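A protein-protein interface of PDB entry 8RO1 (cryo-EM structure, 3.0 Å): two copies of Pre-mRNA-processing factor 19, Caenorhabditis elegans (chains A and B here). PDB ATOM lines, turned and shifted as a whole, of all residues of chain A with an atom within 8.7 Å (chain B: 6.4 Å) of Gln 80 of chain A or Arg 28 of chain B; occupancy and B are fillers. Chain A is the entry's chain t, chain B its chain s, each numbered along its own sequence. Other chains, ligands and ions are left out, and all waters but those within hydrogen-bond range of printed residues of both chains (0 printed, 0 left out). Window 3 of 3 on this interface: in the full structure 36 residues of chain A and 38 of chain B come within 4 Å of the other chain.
The guanidinium group (NH1) of Arg 28 of chain B lies within salt-bridge range of the side-chain carboxylate (OD1) of Asp 84 of chain A (3.1 Å). The side-chain amino group of Lys 32 of chain B lies within salt-bridge range of the side-chain carboxylate of Asp 81 of chain A. The side-chain amino group (NZ) of Lys 32 of chain B lies within salt-bridge range of the side-chain carboxylate (OD2) of Asp 84 of chain A, 3.2 Å away.
OD2 of Asp 26 of chain B is in salt-bridge range of NH2 of Arg 28 of chain B, at 2.7 Å. O of Glu 82 of chain A is in hydrogen-bond range of OG1 of Thr 85 of chain A.
Leu 79 of chain A touches Trp 83 of chain B (O to CH2, 3.3 Å). NH1 of Arg 28 of chain B touches NE2 of Gln 80 of chain A (3.6 Å). Glu 82 of chain A touches Trp 83 of chain B. Trp 83 of chain A touches Arg 28 of chain B (NE1 to NH1, 3.7 Å). N of Trp 83 of chain A touches CH2 of Trp 83 of chain B, at 3.95 Å. Leu 29 of chain B touches Asp 84 of chain A. Leu 88 of chain A touches Leu 29 of chain B (CD2 to O, 3.6 Å). Leu 88 of chain A touches Lys 32 of chain B. CD2 of Leu 88 of chain A touches CD2 of Phe 33 of chain B, at 3.9 Å.
Gln 80 of chain A touches just one residue of chain B: Arg 28 (3.6 Å). Printed residues of chain A within 4 Å of Trp 83 of chain B: Leu 79 (3.3 Å), Glu 82 (3.9 Å) and Trp 83 (3.95 Å). Of the printed residues of chain B, Leu 88 of chain A touches Leu 29 (3.6 Å), Lys 32 (3.7 Å) and Phe 33 (3.9 Å). The nearest residue of chain A that does not touch Arg 28 of chain B is Leu 88 of chain A (5.9 Å).
Of the 13 printed residues of chain B, 5 touch a printed residue of chain A. Of the 16 printed residues of chain A, 7 touch a printed residue of chain B. Hydrophobic or aromatic side chains of chain A that line the printed part of chain B: Leu 79, Trp 83 and Leu 88. Among the printed residues, 12 pairs touch across the chains.
Trp 83 of chain B touches its own counterpart, Trp 83 of chain A.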
ATOM      1  N   PRO A  73      12.646 -28.658  37.530  1.00  0.00           N
ATOM      2  CA  PRO A  73      12.464 -27.299  36.997  1.00  0.00           C
ATOM      3  C   PRO A  73      13.652 -26.785  36.202  1.00  0.00           C
ATOM      4  O   PRO A  73      13.456 -26.007  35.264  1.00  0.00           O
ATOM      5  CB  PRO A  73      12.229 -26.459  38.257  1.00  0.00           C
ATOM      6  CG  PRO A  73      11.737 -27.391  39.239  1.00  0.00           C
ATOM      7  CD  PRO A  73      12.455 -28.661  38.986  1.00  0.00           C
ATOM      8  N   SER A  74      14.876 -27.180  36.550  1.00  0.00           N
ATOM      9  CA  SER A  74      16.021 -26.769  35.748  1.00  0.00           C
ATOM     10  C   SER A  74      15.990 -27.411  34.364  1.00  0.00           C
ATOM     11  O   SER A  74      16.337 -26.766  33.371  1.00  0.00           O
ATOM     12  CB  SER A  74      17.322 -27.109  36.469  1.00  0.00           C
ATOM     13  OG  SER A  74      17.574 -28.497  36.447  1.00  0.00           O
ATOM     14  N   LEU A  75      15.580 -28.680  34.276  1.00  0.00           N
ATOM     15  CA  LEU A  75      15.483 -29.341  32.976  1.00  0.00           C
ATOM     16  C   LEU A  75      14.350 -28.779  32.132  1.00  0.00           C
ATOM     17  O   LEU A  75      14.481 -28.674  30.910  1.00  0.00           O
ATOM     18  CB  LEU A  75      15.313 -30.845  33.145  1.00  0.00           C
ATOM     19  CG  LEU A  75      16.425 -31.619  33.844  1.00  0.00           C
ATOM     20  CD1 LEU A  75      16.025 -33.070  33.966  1.00  0.00           C
ATOM     21  CD2 LEU A  75      17.740 -31.509  33.100  1.00  0.00           C
ATOM     22  N   LEU A  76      13.219 -28.443  32.746  1.00  0.00           N
ATOM     23  CA  LEU A  76      12.148 -27.822  31.976  1.00  0.00           C
ATOM     24  C   LEU A  76      12.571 -26.461  31.443  1.00  0.00           C
ATOM     25  O   LEU A  76      12.187 -26.083  30.332  1.00  0.00           O
ATOM     26  CB  LEU A  76      10.882 -27.711  32.818  1.00  0.00           C
ATOM     27  CG  LEU A  76      10.261 -29.015  33.328  1.00  0.00           C
ATOM     28  CD1 LEU A  76       9.078 -28.711  34.214  1.00  0.00           C
ATOM     29  CD2 LEU A  76       9.806 -29.905  32.202  1.00  0.00           C
ATOM     30  N   LYS A  77      13.337 -25.699  32.222  1.00  0.00           N
ATOM     31  CA  LYS A  77      13.879 -24.449  31.705  1.00  0.00           C
ATOM     32  C   LYS A  77      14.842 -24.696  30.558  1.00  0.00           C
ATOM     33  O   LYS A  77      14.898 -23.909  29.609  1.00  0.00           O
ATOM     34  CB  LYS A  77      14.592 -23.676  32.812  1.00  0.00           C
ATOM     35  CG  LYS A  77      13.707 -22.932  33.797  1.00  0.00           C
ATOM     36  CD  LYS A  77      12.944 -21.785  33.146  1.00  0.00           C
ATOM     37  CE  LYS A  77      12.186 -20.971  34.175  1.00  0.00           C
ATOM     38  NZ  LYS A  77      13.112 -20.094  34.945  1.00  0.00           N
ATOM     39  N   MET A  78      15.619 -25.776  30.628  1.00  0.00           N
ATOM     40  CA  MET A  78      16.474 -26.133  29.502  1.00  0.00           C
ATOM     41  C   MET A  78      15.658 -26.423  28.250  1.00  0.00           C
ATOM     42  O   MET A  78      15.944 -25.885  27.178  1.00  0.00           O
ATOM     43  CB  MET A  78      17.351 -27.331  29.855  1.00  0.00           C
ATOM     44  CG  MET A  78      18.492 -27.013  30.792  1.00  0.00           C
ATOM     45  SD  MET A  78      19.424 -28.483  31.252  1.00  0.00           S
ATOM     46  CE  MET A  78      20.448 -27.839  32.570  1.00  0.00           C
ATOM     47  N   LEU A  79      14.627 -27.259  28.362  1.00  0.00           N
ATOM     48  CA  LEU A  79      13.775 -27.521  27.206  1.00  0.00           C
ATOM     49  C   LEU A  79      13.044 -26.267  26.747  1.00  0.00           C
ATOM     50  O   LEU A  79      12.882 -26.045  25.544  1.00  0.00           O
ATOM     51  CB  LEU A  79      12.784 -28.638  27.526  1.00  0.00           C
ATOM     52  CG  LEU A  79      13.318 -30.064  27.667  1.00  0.00           C
ATOM     53  CD1 LEU A  79      12.179 -30.999  27.949  1.00  0.00           C
ATOM     54  CD2 LEU A  79      14.058 -30.525  26.426  1.00  0.00           C
ATOM     55  N   GLN A  80      12.565 -25.453  27.682  1.00  0.00           N
ATOM     56  CA  GLN A  80      11.908 -24.205  27.305  1.00  0.00           C
ATOM     57  C   GLN A  80      12.865 -23.251  26.604  1.00  0.00           C
ATOM     58  O   GLN A  80      12.467 -22.532  25.682  1.00  0.00           O
ATOM     59  CB  GLN A  80      11.299 -23.533  28.526  1.00  0.00           C
ATOM     60  CG  GLN A  80      10.323 -22.432  28.175  1.00  0.00           C
ATOM     61  CD  GLN A  80       9.541 -21.943  29.371  1.00  0.00           C
ATOM     62  OE1 GLN A  80      10.082 -21.793  30.465  1.00  0.00           O
ATOM     63  NE2 GLN A  80       8.255 -21.688  29.169  1.00  0.00           N
ATOM     64  N   ASP A  81      14.126 -23.210  27.039  1.00  0.00           N
ATOM     65  CA  ASP A  81      15.114 -22.370  26.367  1.00  0.00           C
ATOM     66  C   ASP A  81      15.353 -22.818  24.933  1.00  0.00           C
ATOM     67  O   ASP A  81      15.414 -21.987  24.023  1.00  0.00           O
ATOM     68  CB  ASP A  81      16.435 -22.389  27.137  1.00  0.00           C
ATOM     69  CG  ASP A  81      16.456 -21.427  28.315  1.00  0.00           C
ATOM     70  OD1 ASP A  81      15.714 -20.424  28.312  1.00  0.00           O
ATOM     71  OD2 ASP A  81      17.233 -21.677  29.260  1.00  0.00           O
ATOM     72  N   GLU A  82      15.484 -24.123  24.707  1.00  0.00           N
ATOM     73  CA  GLU A  82      15.665 -24.618  23.349  1.00  0.00           C
ATOM     74  C   GLU A  82      14.453 -24.312  22.486  1.00  0.00           C
ATOM     75  O   GLU A  82      14.594 -23.931  21.322  1.00  0.00           O
ATOM     76  CB  GLU A  82      15.934 -26.119  23.361  1.00  0.00           C
ATOM     77  CG  GLU A  82      17.192 -26.558  24.100  1.00  0.00           C
ATOM     78  CD  GLU A  82      18.453 -25.866  23.621  1.00  0.00           C
ATOM     79  OE1 GLU A  82      18.552 -25.578  22.411  1.00  0.00           O
ATOM     80  OE2 GLU A  82      19.352 -25.622  24.452  1.00  0.00           O
ATOM     81  N   TRP A  83      13.256 -24.496  23.036  1.00  0.00           N
ATOM     82  CA  TRP A  83      12.032 -24.172  22.312  1.00  0.00           C
ATOM     83  C   TRP A  83      11.998 -22.720  21.857  1.00  0.00           C
ATOM     84  O   TRP A  83      11.561 -22.433  20.738  1.00  0.00           O
ATOM     85  CB  TRP A  83      10.829 -24.478  23.201  1.00  0.00           C
ATOM     86  CG  TRP A  83       9.618 -23.660  22.945  1.00  0.00           C
ATOM     87  CD1 TRP A  83       9.245 -22.515  23.587  1.00  0.00           C
ATOM     88  CD2 TRP A  83       8.596 -23.940  22.006  1.00  0.00           C
ATOM     89  NE1 TRP A  83       8.059 -22.059  23.086  1.00  0.00           N
ATOM     90  CE2 TRP A  83       7.637 -22.921  22.114  1.00  0.00           C
ATOM     91  CE3 TRP A  83       8.401 -24.952  21.075  1.00  0.00           C
ATOM     92  CZ2 TRP A  83       6.503 -22.890  21.329  1.00  0.00           C
ATOM     93  CZ3 TRP A  83       7.274 -24.923  20.303  1.00  0.00           C
ATOM     94  CH2 TRP A  83       6.339 -23.898  20.429  1.00  0.00           C
ATOM     95  N   ASP A  84      12.411 -21.791  22.718  1.00  0.00           N
ATOM     96  CA  ASP A  84      12.423 -20.381  22.334  1.00  0.00           C
ATOM     97  C   ASP A  84      13.321 -20.121  21.129  1.00  0.00           C
ATOM     98  O   ASP A  84      12.958 -19.353  20.235  1.00  0.00           O
ATOM     99  CB  ASP A  84      12.853 -19.513  23.517  1.00  0.00           C
ATOM    100  CG  ASP A  84      11.793 -19.436  24.609  1.00  0.00           C
ATOM    101  OD1 ASP A  84      10.633 -19.821  24.357  1.00  0.00           O
ATOM    102  OD2 ASP A  84      12.118 -18.974  25.724  1.00  0.00           O
ATOM    103  N   THR A  85      14.492 -20.749  21.082  1.00  0.00           N
ATOM    104  CA  THR A  85      15.376 -20.547  19.938  1.00  0.00           C
ATOM    105  C   THR A  85      14.812 -21.152  18.658  1.00  0.00           C
ATOM    106  O   THR A  85      14.972 -20.575  17.577  1.00  0.00           O
ATOM    107  CB  THR A  85      16.758 -21.123  20.229  1.00  0.00           C
ATOM    108  OG1 THR A  85      16.680 -22.548  20.311  1.00  0.00           O
ATOM    109  CG2 THR A  85      17.323 -20.553  21.516  1.00  0.00           C
ATOM    110  N   VAL A  86      14.154 -22.305  18.745  1.00  0.00           N
ATOM    111  CA  VAL A  86      13.546 -22.888  17.553  1.00  0.00           C
ATOM    112  C   VAL A  86      12.422 -22.001  17.045  1.00  0.00           C
ATOM    113  O   VAL A  86      12.252 -21.830  15.835  1.00  0.00           O
ATOM    114  CB  VAL A  86      13.059 -24.319  17.829  1.00  0.00           C
ATOM    115  CG1 VAL A  86      12.297 -24.890  16.615  1.00  0.00           C
ATOM    116  CG2 VAL A  86      14.250 -25.199  18.168  1.00  0.00           C
ATOM    117  N   MET A  87      11.637 -21.425  17.949  1.00  0.00           N
ATOM    118  CA  MET A  87      10.568 -20.536  17.515  1.00  0.00           C
ATOM    119  C   MET A  87      11.118 -19.251  16.920  1.00  0.00           C
ATOM    120  O   MET A  87      10.607 -18.770  15.903  1.00  0.00           O
ATOM    121  CB  MET A  87       9.636 -20.236  18.685  1.00  0.00           C
ATOM    122  CG  MET A  87       8.747 -21.404  19.082  1.00  0.00           C
ATOM    123  SD  MET A  87       7.577 -21.925  17.810  1.00  0.00           S
ATOM    124  CE  MET A  87       8.373 -23.399  17.177  1.00  0.00           C
ATOM    125  N   LEU A  88      12.133 -18.658  17.542  1.00  0.00           N
ATOM    126  CA  LEU A  88      12.725 -17.452  16.974  1.00  0.00           C
ATOM    127  C   LEU A  88      13.385 -17.727  15.627  1.00  0.00           C
ATOM    128  O   LEU A  88      13.332 -16.887  14.724  1.00  0.00           O
ATOM    129  CB  LEU A  88      13.733 -16.852  17.951  1.00  0.00           C
ATOM    130  CG  LEU A  88      13.131 -16.219  19.205  1.00  0.00           C
ATOM    131  CD1 LEU A  88      14.177 -16.088  20.292  1.00  0.00           C
ATOM    132  CD2 LEU A  88      12.507 -14.869  18.904  1.00  0.00           C
ATOM    133  N   THR B  12      -0.126 -17.525  25.002  1.00  0.00           N
ATOM    134  CA  THR B  12       0.818 -16.885  25.907  1.00  0.00           C
ATOM    135  C   THR B  12       0.130 -16.541  27.213  1.00  0.00           C
ATOM    136  O   THR B  12      -1.006 -16.058  27.230  1.00  0.00           O
ATOM    137  CB  THR B  12       1.421 -15.612  25.292  1.00  0.00           C
ATOM    138  OG1 THR B  12       2.143 -14.893  26.297  1.00  0.00           O
ATOM    139  CG2 THR B  12       0.345 -14.699  24.696  1.00  0.00           C
ATOM    140  N   GLU B  13       0.846 -16.785  28.307  1.00  0.00           N
ATOM    141  CA  GLU B  13       0.430 -16.365  29.636  1.00  0.00           C
ATOM    142  C   GLU B  13       0.784 -14.919  29.951  1.00  0.00           C
ATOM    143  O   GLU B  13       0.325 -14.407  30.977  1.00  0.00           O
ATOM    144  CB  GLU B  13       1.065 -17.271  30.693  1.00  0.00           C
ATOM    145  CG  GLU B  13       0.887 -18.764  30.436  1.00  0.00           C
ATOM    146  CD  GLU B  13       2.043 -19.374  29.657  1.00  0.00           C
ATOM    147  OE1 GLU B  13       2.702 -18.634  28.895  1.00  0.00           O
ATOM    148  OE2 GLU B  13       2.295 -20.588  29.808  1.00  0.00           O
ATOM    149  N   ASP B  14       1.575 -14.253  29.111  1.00  0.00           N
ATOM    150  CA  ASP B  14       2.123 -12.932  29.419  1.00  0.00           C
ATOM    151  C   ASP B  14       2.161 -12.111  28.140  1.00  0.00           C
ATOM    152  O   ASP B  14       3.233 -11.807  27.605  1.00  0.00           O
ATOM    153  CB  ASP B  14       3.519 -13.074  30.029  1.00  0.00           C
ATOM    154  CG  ASP B  14       4.054 -11.772  30.595  1.00  0.00           C
ATOM    155  OD1 ASP B  14       3.256 -10.850  30.866  1.00  0.00           O
ATOM    156  OD2 ASP B  14       5.286 -11.669  30.770  1.00  0.00           O
ATOM    157  N   VAL B  16       2.238  -9.120  25.491  1.00  0.00           N
ATOM    158  CA  VAL B  16       2.840  -7.797  25.483  1.00  0.00           C
ATOM    159  C   VAL B  16       2.745  -7.270  24.056  1.00  0.00           C
ATOM    160  O   VAL B  16       2.655  -8.038  23.096  1.00  0.00           O
ATOM    161  CB  VAL B  16       4.295  -7.868  26.028  1.00  0.00           C
ATOM    162  CG1 VAL B  16       5.295  -8.400  24.982  1.00  0.00           C
ATOM    163  CG2 VAL B  16       4.745  -6.549  26.605  1.00  0.00           C
ATOM    164  N   ASP B  26       4.507 -12.856  23.153  1.00  0.00           N
ATOM    165  CA  ASP B  26       4.917 -13.396  24.445  1.00  0.00           C
ATOM    166  C   ASP B  26       6.205 -12.726  24.899  1.00  0.00           C
ATOM    167  O   ASP B  26       7.179 -12.677  24.145  1.00  0.00           O
ATOM    168  CB  ASP B  26       5.111 -14.908  24.352  1.00  0.00           C
ATOM    169  CG  ASP B  26       5.172 -15.580  25.711  1.00  0.00           C
ATOM    170  OD1 ASP B  26       4.836 -14.935  26.724  1.00  0.00           O
ATOM    171  OD2 ASP B  26       5.552 -16.768  25.766  1.00  0.00           O
ATOM    172  N   ARG B  27       6.196 -12.213  26.134  1.00  0.00           N
ATOM    173  CA  ARG B  27       7.249 -11.316  26.616  1.00  0.00           C
ATOM    174  C   ARG B  27       8.657 -11.890  26.490  1.00  0.00           C
ATOM    175  O   ARG B  27       9.550 -11.229  25.955  1.00  0.00           O
ATOM    176  CB  ARG B  27       6.977 -10.916  28.070  1.00  0.00           C
ATOM    177  CG  ARG B  27       7.875  -9.769  28.573  1.00  0.00           C
ATOM    178  CD  ARG B  27       7.720  -9.499  30.055  1.00  0.00           C
ATOM    179  NE  ARG B  27       6.331  -9.235  30.412  1.00  0.00           N
ATOM    180  CZ  ARG B  27       5.740  -8.044  30.390  1.00  0.00           C
ATOM    181  NH1 ARG B  27       4.444  -7.963  30.673  1.00  0.00           N
ATOM    182  NH2 ARG B  27       6.410  -6.931  30.125  1.00  0.00           N
ATOM    183  N   ARG B  28       8.882 -13.118  26.962  1.00  0.00           N
ATOM    184  CA  ARG B  28      10.241 -13.654  26.910  1.00  0.00           C
ATOM    185  C   ARG B  28      10.729 -13.866  25.484  1.00  0.00           C
ATOM    186  O   ARG B  28      11.935 -13.793  25.230  1.00  0.00           O
ATOM    187  CB  ARG B  28      10.327 -14.959  27.705  1.00  0.00           C
ATOM    188  CG  ARG B  28       9.683 -16.180  27.062  1.00  0.00           C
ATOM    189  CD  ARG B  28       9.789 -17.390  27.966  1.00  0.00           C
ATOM    190  NE  ARG B  28       9.398 -18.610  27.272  1.00  0.00           N
ATOM    191  CZ  ARG B  28       8.164 -18.914  26.890  1.00  0.00           C
ATOM    192  NH1 ARG B  28       7.981 -19.929  26.051  1.00  0.00           N
ATOM    193  NH2 ARG B  28       7.105 -18.297  27.392  1.00  0.00           N
ATOM    194  N   LEU B  29       9.823 -14.133  24.547  1.00  0.00           N
ATOM    195  CA  LEU B  29      10.231 -14.339  23.163  1.00  0.00           C
ATOM    196  C   LEU B  29      10.611 -13.028  22.482  1.00  0.00           C
ATOM    197  O   LEU B  29      11.663 -12.933  21.841  1.00  0.00           O
ATOM    198  CB  LEU B  29       9.115 -15.049  22.398  1.00  0.00           C
ATOM    199  CG  LEU B  29       8.924 -16.542  22.679  1.00  0.00           C
ATOM    200  CD1 LEU B  29       7.698 -17.028  21.937  1.00  0.00           C
ATOM    201  CD2 LEU B  29      10.150 -17.360  22.284  1.00  0.00           C
ATOM    202  N   ILE B  30       9.772 -12.000  22.619  1.00  0.00           N
ATOM    203  CA  ILE B  30      10.044 -10.719  21.969  1.00  0.00           C
ATOM    204  C   ILE B  30      11.283 -10.057  22.561  1.00  0.00           C
ATOM    205  O   ILE B  30      12.038  -9.388  21.848  1.00  0.00           O
ATOM    206  CB  ILE B  30       8.797  -9.805  22.024  1.00  0.00           C
ATOM    207  CG1 ILE B  30       9.026  -8.463  21.306  1.00  0.00           C
ATOM    208  CG2 ILE B  30       8.333  -9.522  23.459  1.00  0.00           C
ATOM    209  CD1 ILE B  30       9.337  -8.586  19.826  1.00  0.00           C
ATOM    210  N   VAL B  31      11.504 -10.211  23.867  1.00  0.00           N
ATOM    211  CA  VAL B  31      12.715  -9.677  24.488  1.00  0.00           C
ATOM    212  C   VAL B  31      13.962 -10.314  23.887  1.00  0.00           C
ATOM    213  O   VAL B  31      14.951  -9.624  23.615  1.00  0.00           O
ATOM    214  CB  VAL B  31      12.656  -9.864  26.016  1.00  0.00           C
ATOM    215  CG1 VAL B  31      14.034  -9.616  26.655  1.00  0.00           C
ATOM    216  CG2 VAL B  31      11.630  -8.894  26.613  1.00  0.00           C
ATOM    217  N   LYS B  32      13.950 -11.627  23.678  1.00  0.00           N
ATOM    218  CA  LYS B  32      15.084 -12.251  23.006  1.00  0.00           C
ATOM    219  C   LYS B  32      15.228 -11.784  21.567  1.00  0.00           C
ATOM    220  O   LYS B  32      16.351 -11.675  21.064  1.00  0.00           O
ATOM    221  CB  LYS B  32      14.948 -13.765  23.037  1.00  0.00           C
ATOM    222  CG  LYS B  32      15.241 -14.360  24.379  1.00  0.00           C
ATOM    223  CD  LYS B  32      14.945 -15.833  24.384  1.00  0.00           C
ATOM    224  CE  LYS B  32      15.246 -16.435  25.733  1.00  0.00           C
ATOM    225  NZ  LYS B  32      15.107 -17.909  25.699  1.00  0.00           N
ATOM    226  N   PHE B  33      14.118 -11.497  20.890  1.00  0.00           N
ATOM    227  CA  PHE B  33      14.205 -10.930  19.550  1.00  0.00           C
ATOM    228  C   PHE B  33      14.823  -9.540  19.592  1.00  0.00           C
ATOM    229  O   PHE B  33      15.716  -9.221  18.800  1.00  0.00           O
ATOM    230  CB  PHE B  33      12.814 -10.895  18.920  1.00  0.00           C
ATOM    231  CG  PHE B  33      12.822 -10.658  17.447  1.00  0.00           C
ATOM    232  CD1 PHE B  33      12.834  -9.376  16.945  1.00  0.00           C
ATOM    233  CD2 PHE B  33      12.818 -11.718  16.562  1.00  0.00           C
ATOM    234  CE1 PHE B  33      12.849  -9.152  15.597  1.00  0.00           C
ATOM    235  CE2 PHE B  33      12.824 -11.500  15.206  1.00  0.00           C
ATOM    236  CZ  PHE B  33      12.833 -10.214  14.721  1.00  0.00           C
ATOM    237  N   TRP B  83       8.029 -32.804  19.954  1.00  0.00           N
ATOM    238  CA  TRP B  83       9.288 -32.162  19.595  1.00  0.00           C
ATOM    239  C   TRP B  83       9.771 -32.566  18.207  1.00  0.00           C
ATOM    240  O   TRP B  83      10.278 -31.726  17.459  1.00  0.00           O
ATOM    241  CB  TRP B  83      10.350 -32.458  20.651  1.00  0.00           C
ATOM    242  CG  TRP B  83      11.387 -31.401  20.665  1.00  0.00           C
ATOM    243  CD1 TRP B  83      12.288 -31.107  19.684  1.00  0.00           C
ATOM    244  CD2 TRP B  83      11.598 -30.443  21.700  1.00  0.00           C
ATOM    245  NE1 TRP B  83      13.046 -30.023  20.048  1.00  0.00           N
ATOM    246  CE2 TRP B  83      12.642 -29.600  21.284  1.00  0.00           C
ATOM    247  CE3 TRP B  83      11.007 -30.219  22.941  1.00  0.00           C
ATOM    248  CZ2 TRP B  83      13.113 -28.561  22.067  1.00  0.00           C
ATOM    249  CZ3 TRP B  83      11.475 -29.189  23.713  1.00  0.00           C
ATOM    250  CH2 TRP B  83      12.516 -28.371  23.275  1.00  0.00           C
